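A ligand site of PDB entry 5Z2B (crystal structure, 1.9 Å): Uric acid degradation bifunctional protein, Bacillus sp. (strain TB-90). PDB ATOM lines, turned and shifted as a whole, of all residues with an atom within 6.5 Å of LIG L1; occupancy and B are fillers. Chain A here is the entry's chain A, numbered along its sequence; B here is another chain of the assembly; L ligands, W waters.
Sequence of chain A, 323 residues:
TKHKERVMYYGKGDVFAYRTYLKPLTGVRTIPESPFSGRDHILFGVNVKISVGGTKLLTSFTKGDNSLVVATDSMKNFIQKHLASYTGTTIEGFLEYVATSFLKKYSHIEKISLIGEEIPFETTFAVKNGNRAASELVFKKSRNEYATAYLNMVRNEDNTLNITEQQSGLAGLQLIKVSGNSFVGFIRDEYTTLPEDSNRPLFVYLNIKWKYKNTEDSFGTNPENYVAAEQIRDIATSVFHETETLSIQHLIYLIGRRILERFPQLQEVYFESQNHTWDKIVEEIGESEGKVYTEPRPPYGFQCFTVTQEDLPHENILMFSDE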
ATOM      1  N   SER A 182     -18.932  26.317  -2.457  1.00  0.00           N
ATOM      2  CA  SER A 182     -19.036  26.979  -3.748  1.00  0.00           C
ATOM      3  C   SER A 182     -20.498  27.012  -4.176  1.00  0.00           C
ATOM      4  O   SER A 182     -21.331  26.227  -3.726  1.00  0.00           O
ATOM      5  CB  SER A 182     -18.172  26.261  -4.822  1.00  0.00           C
ATOM      6  OG  SER A 182     -18.788  25.056  -5.276  1.00  0.00           O
ATOM      7  N   PHE A 183     -20.800  27.982  -5.030  1.00  0.00           N
ATOM      8  CA  PHE A 183     -22.060  27.989  -5.761  1.00  0.00           C
ATOM      9  C   PHE A 183     -21.711  28.497  -7.159  1.00  0.00           C
ATOM     10  O   PHE A 183     -21.538  29.690  -7.379  1.00  0.00           O
ATOM     11  CB  PHE A 183     -23.121  28.851  -5.072  1.00  0.00           C
ATOM     12  CG  PHE A 183     -24.476  28.718  -5.695  1.00  0.00           C
ATOM     13  CD1 PHE A 183     -25.067  27.469  -5.807  1.00  0.00           C
ATOM     14  CD2 PHE A 183     -25.139  29.813  -6.196  1.00  0.00           C
ATOM     15  CE1 PHE A 183     -26.304  27.318  -6.386  1.00  0.00           C
ATOM     16  CE2 PHE A 183     -26.371  29.677  -6.791  1.00  0.00           C
ATOM     17  CZ  PHE A 183     -26.958  28.424  -6.886  1.00  0.00           C
ATOM     18  N   PHE A 186     -24.812  27.686 -12.042  1.00  0.00           N
ATOM     19  CA  PHE A 186     -26.244  27.899 -12.111  1.00  0.00           C
ATOM     20  C   PHE A 186     -26.609  28.692 -13.371  1.00  0.00           C
ATOM     21  O   PHE A 186     -25.754  29.203 -14.098  1.00  0.00           O
ATOM     22  CB  PHE A 186     -26.747  28.629 -10.855  1.00  0.00           C
ATOM     23  CG  PHE A 186     -25.984  29.857 -10.505  1.00  0.00           C
ATOM     24  CD1 PHE A 186     -26.361  31.085 -11.022  1.00  0.00           C
ATOM     25  CD2 PHE A 186     -24.889  29.795  -9.664  1.00  0.00           C
ATOM     26  CE1 PHE A 186     -25.667  32.224 -10.691  1.00  0.00           C
ATOM     27  CE2 PHE A 186     -24.185  30.944  -9.332  1.00  0.00           C
ATOM     28  CZ  PHE A 186     -24.574  32.155  -9.856  1.00  0.00           C
ATOM     29  N   LEU A 194     -26.199  37.369  -9.891  1.00  0.00           N
ATOM     30  CA  LEU A 194     -25.350  36.771  -8.861  1.00  0.00           C
ATOM     31  C   LEU A 194     -24.040  36.257  -9.469  1.00  0.00           C
ATOM     32  O   LEU A 194     -24.082  35.409 -10.361  1.00  0.00           O
ATOM     33  CB  LEU A 194     -26.082  35.620  -8.180  1.00  0.00           C
ATOM     34  CG  LEU A 194     -25.380  34.959  -6.995  1.00  0.00           C
ATOM     35  CD1 LEU A 194     -25.340  35.907  -5.799  1.00  0.00           C
ATOM     36  CD2 LEU A 194     -26.038  33.648  -6.617  1.00  0.00           C
ATOM     37  N   ARG A 200     -17.331  30.705  -0.750  1.00  0.00           N
ATOM     38  CA  ARG A 200     -18.199  31.608  -0.013  1.00  0.00           C
ATOM     39  C   ARG A 200     -18.355  31.150   1.424  1.00  0.00           C
ATOM     40  O   ARG A 200     -18.292  29.948   1.721  1.00  0.00           O
ATOM     41  CB  ARG A 200     -19.586  31.667  -0.661  1.00  0.00           C
ATOM     42  CG  ARG A 200     -20.305  30.308  -0.695  1.00  0.00           C
ATOM     43  CD  ARG A 200     -21.675  30.398  -1.321  1.00  0.00           C
ATOM     44  NE  ARG A 200     -22.382  29.116  -1.290  1.00  0.00           N
ATOM     45  CZ  ARG A 200     -23.666  28.976  -1.608  1.00  0.00           C
ATOM     46  NH1 ARG A 200     -24.348  30.040  -1.961  1.00  0.00           N
ATOM     47  NH2 ARG A 200     -24.262  27.784  -1.560  1.00  0.00           N
ATOM     48  N   LEU A 202     -20.679  30.159   3.479  1.00  0.00           N
ATOM     49  CA  LEU A 202     -22.076  29.753   3.447  1.00  0.00           C
ATOM     50  C   LEU A 202     -22.684  29.780   4.840  1.00  0.00           C
ATOM     51  O   LEU A 202     -22.183  29.127   5.767  1.00  0.00           O
ATOM     52  CB  LEU A 202     -22.204  28.349   2.845  1.00  0.00           C
ATOM     53  CG  LEU A 202     -23.593  27.699   2.922  1.00  0.00           C
ATOM     54  CD1 LEU A 202     -24.667  28.573   2.296  1.00  0.00           C
ATOM     55  CD2 LEU A 202     -23.606  26.336   2.226  1.00  0.00           C
ATOM     56  N   LEU A 246     -21.446  22.331  -2.696  1.00  0.00           N
ATOM     57  CA  LEU A 246     -21.691  22.838  -4.032  1.00  0.00           C
ATOM     58  C   LEU A 246     -22.969  23.667  -4.106  1.00  0.00           C
ATOM     59  O   LEU A 246     -23.201  24.314  -5.126  1.00  0.00           O
ATOM     60  CB  LEU A 246     -21.771  21.670  -5.024  1.00  0.00           C
ATOM     61  CG  LEU A 246     -20.484  20.848  -5.157  1.00  0.00           C
ATOM     62  CD1 LEU A 246     -20.724  19.580  -5.970  1.00  0.00           C
ATOM     63  CD2 LEU A 246     -19.344  21.686  -5.767  1.00  0.00           C
ATOM     64  N   SER A 247     -23.778  23.653  -3.038  1.00  0.00           N
ATOM     65  CA  SER A 247     -25.034  24.383  -2.874  1.00  0.00           C
ATOM     66  C   SER A 247     -25.576  24.009  -1.501  1.00  0.00           C
ATOM     67  O   SER A 247     -25.083  23.080  -0.852  1.00  0.00           O
ATOM     68  CB  SER A 247     -26.063  24.040  -3.943  1.00  0.00           C
ATOM     69  OG  SER A 247     -26.405  22.672  -3.838  1.00  0.00           O
ATOM     70  N   ILE A 248     -26.596  24.735  -1.053  1.00  0.00           N
ATOM     71  CA  ILE A 248     -27.356  24.297   0.120  1.00  0.00           C
ATOM     72  C   ILE A 248     -28.091  22.989  -0.194  1.00  0.00           C
ATOM     73  O   ILE A 248     -28.099  22.050   0.605  1.00  0.00           O
ATOM     74  CB  ILE A 248     -28.337  25.386   0.586  1.00  0.00           C
ATOM     75  CG1 ILE A 248     -27.579  26.651   0.989  1.00  0.00           C
ATOM     76  CG2 ILE A 248     -29.182  24.862   1.757  1.00  0.00           C
ATOM     77  CD1 ILE A 248     -28.472  27.889   1.158  1.00  0.00           C
ATOM     78  N   GLN A 249     -28.731  22.938  -1.364  1.00  0.00           N
ATOM     79  CA  GLN A 249     -29.360  21.709  -1.833  1.00  0.00           C
ATOM     80  C   GLN A 249     -28.424  20.513  -1.661  1.00  0.00           C
ATOM     81  O   GLN A 249     -28.809  19.469  -1.094  1.00  0.00           O
ATOM     82  CB  GLN A 249     -29.755  21.880  -3.297  1.00  0.00           C
ATOM     83  CG  GLN A 249     -30.876  22.884  -3.519  1.00  0.00           C
ATOM     84  CD  GLN A 249     -30.388  24.276  -3.854  1.00  0.00           C
ATOM     85  OE1 GLN A 249     -29.396  24.762  -3.325  1.00  0.00           O
ATOM     86  NE2 GLN A 249     -31.115  24.938  -4.749  1.00  0.00           N
ATOM     87  N   ASN A 275     -30.857  30.471   3.221  1.00  0.00           N
ATOM     88  CA  ASN A 275     -29.545  31.037   2.897  1.00  0.00           C
ATOM     89  C   ASN A 275     -29.441  32.442   3.493  1.00  0.00           C
ATOM     90  O   ASN A 275     -30.243  33.320   3.144  1.00  0.00           O
ATOM     91  CB  ASN A 275     -29.370  31.109   1.388  1.00  0.00           C
ATOM     92  CG  ASN A 275     -27.965  31.485   0.980  1.00  0.00           C
ATOM     93  OD1 ASN A 275     -27.157  31.973   1.785  1.00  0.00           O
ATOM     94  ND2 ASN A 275     -27.668  31.282  -0.293  1.00  0.00           N
ATOM     95  N   GLY A 301     -32.918  33.029   0.261  1.00  0.00           N
ATOM     96  CA  GLY A 301     -33.217  31.780  -0.408  1.00  0.00           C
ATOM     97  C   GLY A 301     -33.642  30.722   0.582  1.00  0.00           C
ATOM     98  O   GLY A 301     -33.291  30.781   1.766  1.00  0.00           O
ATOM     99  N   PHE A 302     -34.384  29.725   0.096  1.00  0.00           N
ATOM    100  CA  PHE A 302     -34.713  28.596   0.946  1.00  0.00           C
ATOM    101  C   PHE A 302     -34.829  27.329   0.101  1.00  0.00           C
ATOM    102  O   PHE A 302     -35.006  27.376  -1.117  1.00  0.00           O
ATOM    103  CB  PHE A 302     -36.003  28.832   1.762  1.00  0.00           C
ATOM    104  CG  PHE A 302     -37.245  29.051   0.928  1.00  0.00           C
ATOM    105  CD1 PHE A 302     -37.986  27.969   0.463  1.00  0.00           C
ATOM    106  CD2 PHE A 302     -37.695  30.331   0.657  1.00  0.00           C
ATOM    107  CE1 PHE A 302     -39.141  28.175  -0.277  1.00  0.00           C
ATOM    108  CE2 PHE A 302     -38.841  30.537  -0.073  1.00  0.00           C
ATOM    109  CZ  PHE A 302     -39.571  29.457  -0.557  1.00  0.00           C
ATOM    110  N   GLN A 303     -34.712  26.193   0.797  1.00  0.00           N
ATOM    111  CA  GLN A 303     -34.872  24.870   0.202  1.00  0.00           C
ATOM    112  C   GLN A 303     -35.698  23.991   1.131  1.00  0.00           C
ATOM    113  O   GLN A 303     -35.671  24.130   2.358  1.00  0.00           O
ATOM    114  CB  GLN A 303     -33.519  24.195  -0.048  1.00  0.00           C
ATOM    115  CG  GLN A 303     -32.580  24.954  -0.963  1.00  0.00           C
ATOM    116  CD  GLN A 303     -31.986  26.200  -0.343  1.00  0.00           C
ATOM    117  OE1 GLN A 303     -31.922  26.347   0.878  1.00  0.00           O
ATOM    118  NE2 GLN A 303     -31.558  27.137  -1.194  1.00  0.00           N
ATOM    119  N   TYR B  10     -37.604  24.732  -3.802  1.00  0.00           N
ATOM    120  CA  TYR B  10     -36.734  25.788  -3.304  1.00  0.00           C
ATOM    121  C   TYR B  10     -37.286  27.097  -3.831  1.00  0.00           C
ATOM    122  O   TYR B  10     -38.132  27.114  -4.736  1.00  0.00           O
ATOM    123  CB  TYR B  10     -35.255  25.532  -3.691  1.00  0.00           C
ATOM    124  CG  TYR B  10     -34.896  25.906  -5.124  1.00  0.00           C
ATOM    125  CD1 TYR B  10     -35.492  25.270  -6.208  1.00  0.00           C
ATOM    126  CD2 TYR B  10     -33.947  26.875  -5.378  1.00  0.00           C
ATOM    127  CE1 TYR B  10     -35.182  25.610  -7.492  1.00  0.00           C
ATOM    128  CE2 TYR B  10     -33.615  27.226  -6.695  1.00  0.00           C
ATOM    129  CZ  TYR B  10     -34.228  26.592  -7.732  1.00  0.00           C
ATOM    130  OH  TYR B  10     -33.909  26.934  -9.037  1.00  0.00           O
ATOM    131  N   LYS B  12     -37.457  31.768  -2.881  1.00  0.00           N
ATOM    132  CA  LYS B  12     -36.961  33.008  -2.303  1.00  0.00           C
ATOM    133  C   LYS B  12     -38.076  33.640  -1.495  1.00  0.00           C
ATOM    134  O   LYS B  12     -39.214  33.732  -1.982  1.00  0.00           O
ATOM    135  CB  LYS B  12     -36.519  33.952  -3.434  1.00  0.00           C
ATOM    136  CG  LYS B  12     -35.703  35.131  -3.016  1.00  0.00           C
ATOM    137  CD  LYS B  12     -34.300  34.706  -2.586  1.00  0.00           C
ATOM    138  CE  LYS B  12     -33.356  35.877  -2.487  1.00  0.00           C
ATOM    139  NZ  LYS B  12     -31.960  35.407  -2.394  1.00  0.00           N
ATOM    140  N   ASN B  66     -25.834  22.130 -10.686  1.00  0.00           N
ATOM    141  CA  ASN B  66     -26.586  23.367 -10.722  1.00  0.00           C
ATOM    142  C   ASN B  66     -27.000  23.734 -12.135  1.00  0.00           C
ATOM    143  O   ASN B  66     -27.498  24.838 -12.353  1.00  0.00           O
ATOM    144  CB  ASN B  66     -25.768  24.483 -10.077  1.00  0.00           C
ATOM    145  CG  ASN B  66     -25.604  24.270  -8.575  1.00  0.00           C
ATOM    146  OD1 ASN B  66     -26.559  23.899  -7.885  1.00  0.00           O
ATOM    147  ND2 ASN B  66     -24.392  24.484  -8.073  1.00  0.00           N
ATOM    148  N   VAL B  69     -30.477  24.972 -12.095  1.00  0.00           N
ATOM    149  CA  VAL B  69     -30.847  25.812 -10.962  1.00  0.00           C
ATOM    150  C   VAL B  69     -30.974  27.254 -11.442  1.00  0.00           C
ATOM    151  O   VAL B  69     -29.993  27.862 -11.881  1.00  0.00           O
ATOM    152  CB  VAL B  69     -29.846  25.696  -9.810  1.00  0.00           C
ATOM    153  CG1 VAL B  69     -30.182  26.713  -8.725  1.00  0.00           C
ATOM    154  CG2 VAL B  69     -29.884  24.283  -9.240  1.00  0.00           C
ATOM    155  N   VAL B  70     -32.195  27.779 -11.383  1.00  0.00           N
ATOM    156  CA  VAL B  70     -32.422  29.220 -11.333  1.00  0.00           C
ATOM    157  C   VAL B  70     -32.018  29.688  -9.941  1.00  0.00           C
ATOM    158  O   VAL B  70     -32.552  29.205  -8.935  1.00  0.00           O
ATOM    159  CB  VAL B  70     -33.897  29.529 -11.631  1.00  0.00           C
ATOM    160  CG1 VAL B  70     -34.181  31.033 -11.549  1.00  0.00           C
ATOM    161  CG2 VAL B  70     -34.304  28.978 -12.988  1.00  0.00           C
ATOM    162  N   ALA B  71     -31.050  30.583  -9.866  1.00  0.00           N
ATOM    163  CA  ALA B  71     -30.603  31.041  -8.564  1.00  0.00           C
ATOM    164  C   ALA B  71     -31.755  31.739  -7.859  1.00  0.00           C
ATOM    165  O   ALA B  71     -32.555  32.442  -8.469  1.00  0.00           O
ATOM    166  CB  ALA B  71     -29.401  31.978  -8.696  1.00  0.00           C
ATOM    167  N   THR B  72     -31.880  31.494  -6.559  1.00  0.00           N
ATOM    168  CA  THR B  72     -32.928  32.187  -5.817  1.00  0.00           C
ATOM    169  C   THR B  72     -32.724  33.695  -5.902  1.00  0.00           C
ATOM    170  O   THR B  72     -33.691  34.457  -5.929  1.00  0.00           O
ATOM    171  CB  THR B  72     -32.996  31.710  -4.367  1.00  0.00           C
ATOM    172  OG1 THR B  72     -31.822  32.105  -3.637  1.00  0.00           O
ATOM    173  CG2 THR B  72     -33.145  30.223  -4.307  1.00  0.00           C
ATOM    174  N   ASP B  73     -31.472  34.139  -6.006  1.00  0.00           N
ATOM    175  CA  ASP B  73     -31.212  35.547  -6.260  1.00  0.00           C
ATOM    176  C   ASP B  73     -31.858  36.006  -7.560  1.00  0.00           C
ATOM    177  O   ASP B  73     -32.387  37.127  -7.640  1.00  0.00           O
ATOM    178  CB  ASP B  73     -29.712  35.798  -6.262  1.00  0.00           C
ATOM    179  CG  ASP B  73     -29.374  37.255  -6.405  1.00  0.00           C
ATOM    180  OD1 ASP B  73     -29.405  37.960  -5.369  1.00  0.00           O
ATOM    181  OD2 ASP B  73     -29.111  37.696  -7.541  1.00  0.00           O
ATOM    182  N   SER B  74     -31.853  35.147  -8.586  1.00  0.00           N
ATOM    183  CA  SER B  74     -32.457  35.505  -9.865  1.00  0.00           C
ATOM    184  C   SER B  74     -33.984  35.581  -9.760  1.00  0.00           C
ATOM    185  O   SER B  74     -34.608  36.417 -10.416  1.00  0.00           O
ATOM    186  CB  SER B  74     -32.024  34.488 -10.915  1.00  0.00           C
ATOM    187  OG  SER B  74     -30.600  34.380 -10.940  1.00  0.00           O
HETATM  188  N1  LIG L   1     -28.630  27.478  -3.701  1.00  0.00           N
HETATM  189  C1  LIG L   1     -27.560  27.940  -2.982  1.00  0.00           C
HETATM  190  O1  LIG L   1     -26.964  27.215  -2.263  1.00  0.00           O
HETATM  191  N2  LIG L   1     -27.200  29.230  -3.091  1.00  0.00           N
HETATM  192  C2  LIG L   1     -27.843  30.072  -3.887  1.00  0.00           C
HETATM  193  C3  LIG L   1     -28.904  29.621  -4.606  1.00  0.00           C
HETATM  194  C4  LIG L   1     -29.306  28.311  -4.505  1.00  0.00           C
HETATM  195  O2  LIG L   1     -30.229  27.905  -5.132  1.00  0.00           O
HETATM  196  N3  LIG L   1     -29.377  30.657  -5.318  1.00  0.00           N
HETATM  197  N4  LIG L   1     -28.629  31.736  -5.037  1.00  0.00           N
HETATM  198  N5  LIG L   1     -27.679  31.378  -4.152  1.00  0.00           N
HETATM  199  O1  LG2 L   2     -30.039  30.517  -1.555  1.00  0.00           O
HETATM  200  O2  LG2 L   2     -30.767  29.691  -1.894  1.00  0.00           O
HETATM  201  O   HOH W   1     -25.826  32.953  -2.842  1.00  0.00           O
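The backbone NH of Thr 72 of chain B is in hydrogen-bond range of a nitrogen (N3) of LIG L1 (2.9 Å). An oxygen (O1) of LIG L1 sits at hydrogen-bond distance from the guanidinium group of Arg 200, at 2.8 Å. The side-chain amide nitrogen (ND2) of Asn 275 sits at hydrogen-bond distance from an oxygen (O1) of LG2 L2, at 2.8 Å. OG1 of Thr 72 of chain B sits at hydrogen-bond distance from N3 of LIG L1, at 3.3 Å. An oxygen (O2) of LG2 L2 sits at hydrogen-bond distance from the side-chain amide nitrogen of Gln 303, 2.8 Å away. The backbone NH (N) of Ile 248 lies within hydrogen-bond range of an oxygen (O1) of LIG L1 (2.8 Å). An oxygen (O2) of LG2 L2 sits at hydrogen-bond distance from the side-chain hydroxyl (OG1) of Thr 72 of chain B (3.2 Å). OE1 of Gln 249 sits at hydrogen-bond distance from N1 of LIG L1, 2.8 Å away.
A nitrogen (N2) of LIG L1 lies close to an oxygen (O1) of LG2 L2 (3.5 Å).
The backbone carbonyl oxygen (O) of Gly 301 lies within hydrogen-bond range of the backbone NH (N) of Asn 275 (2.9 Å). The side-chain hydroxyl of Ser 247 lies close to the backbone NH of Gln 249, at 3.4 Å. The backbone carbonyl oxygen (O) of Val 70 of chain B lies within hydrogen-bond range of the side-chain hydroxyl (OH) of Tyr 10 of chain B, at 2.6 Å.
Residues that only touch LIG L1: Phe 183 (3.2 Å), Leu 194 (3.6 Å), Ser 247 (3.5 Å), Asn 275 (3.5 Å), Gln 303 (3.9 Å), Tyr 10 of chain B (3.8 Å), Val 69 of chain B (3.8 Å), Ala 71 of chain B (3.5 Å) and Asp 73 of chain B (3.8 Å). Hydrophobic or aromatic side chains that line LIG L1: Phe 183, Leu 194, Ile 248, Tyr 10 of chain B, Val 69 of chain B and Ala 71 of chain B. 13 residues have an atom within 4 Å of LIG L1: Phe 183, Leu 194, Arg 200, Ser 247, Ile 248, Gln 249, Asn 275, Gln 303, Tyr 10 of chain B, Val 69 of chain B, Ala 71 of chain B, Thr 72 of chain B and Asp 73 of chain B. Along chain A the residues within 4 Å of LIG L1 span positions 183 to 303.
Water W1 bridges a nitrogen (N5) of LIG L1 and the guanidinium group (NH1) of Arg 200.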
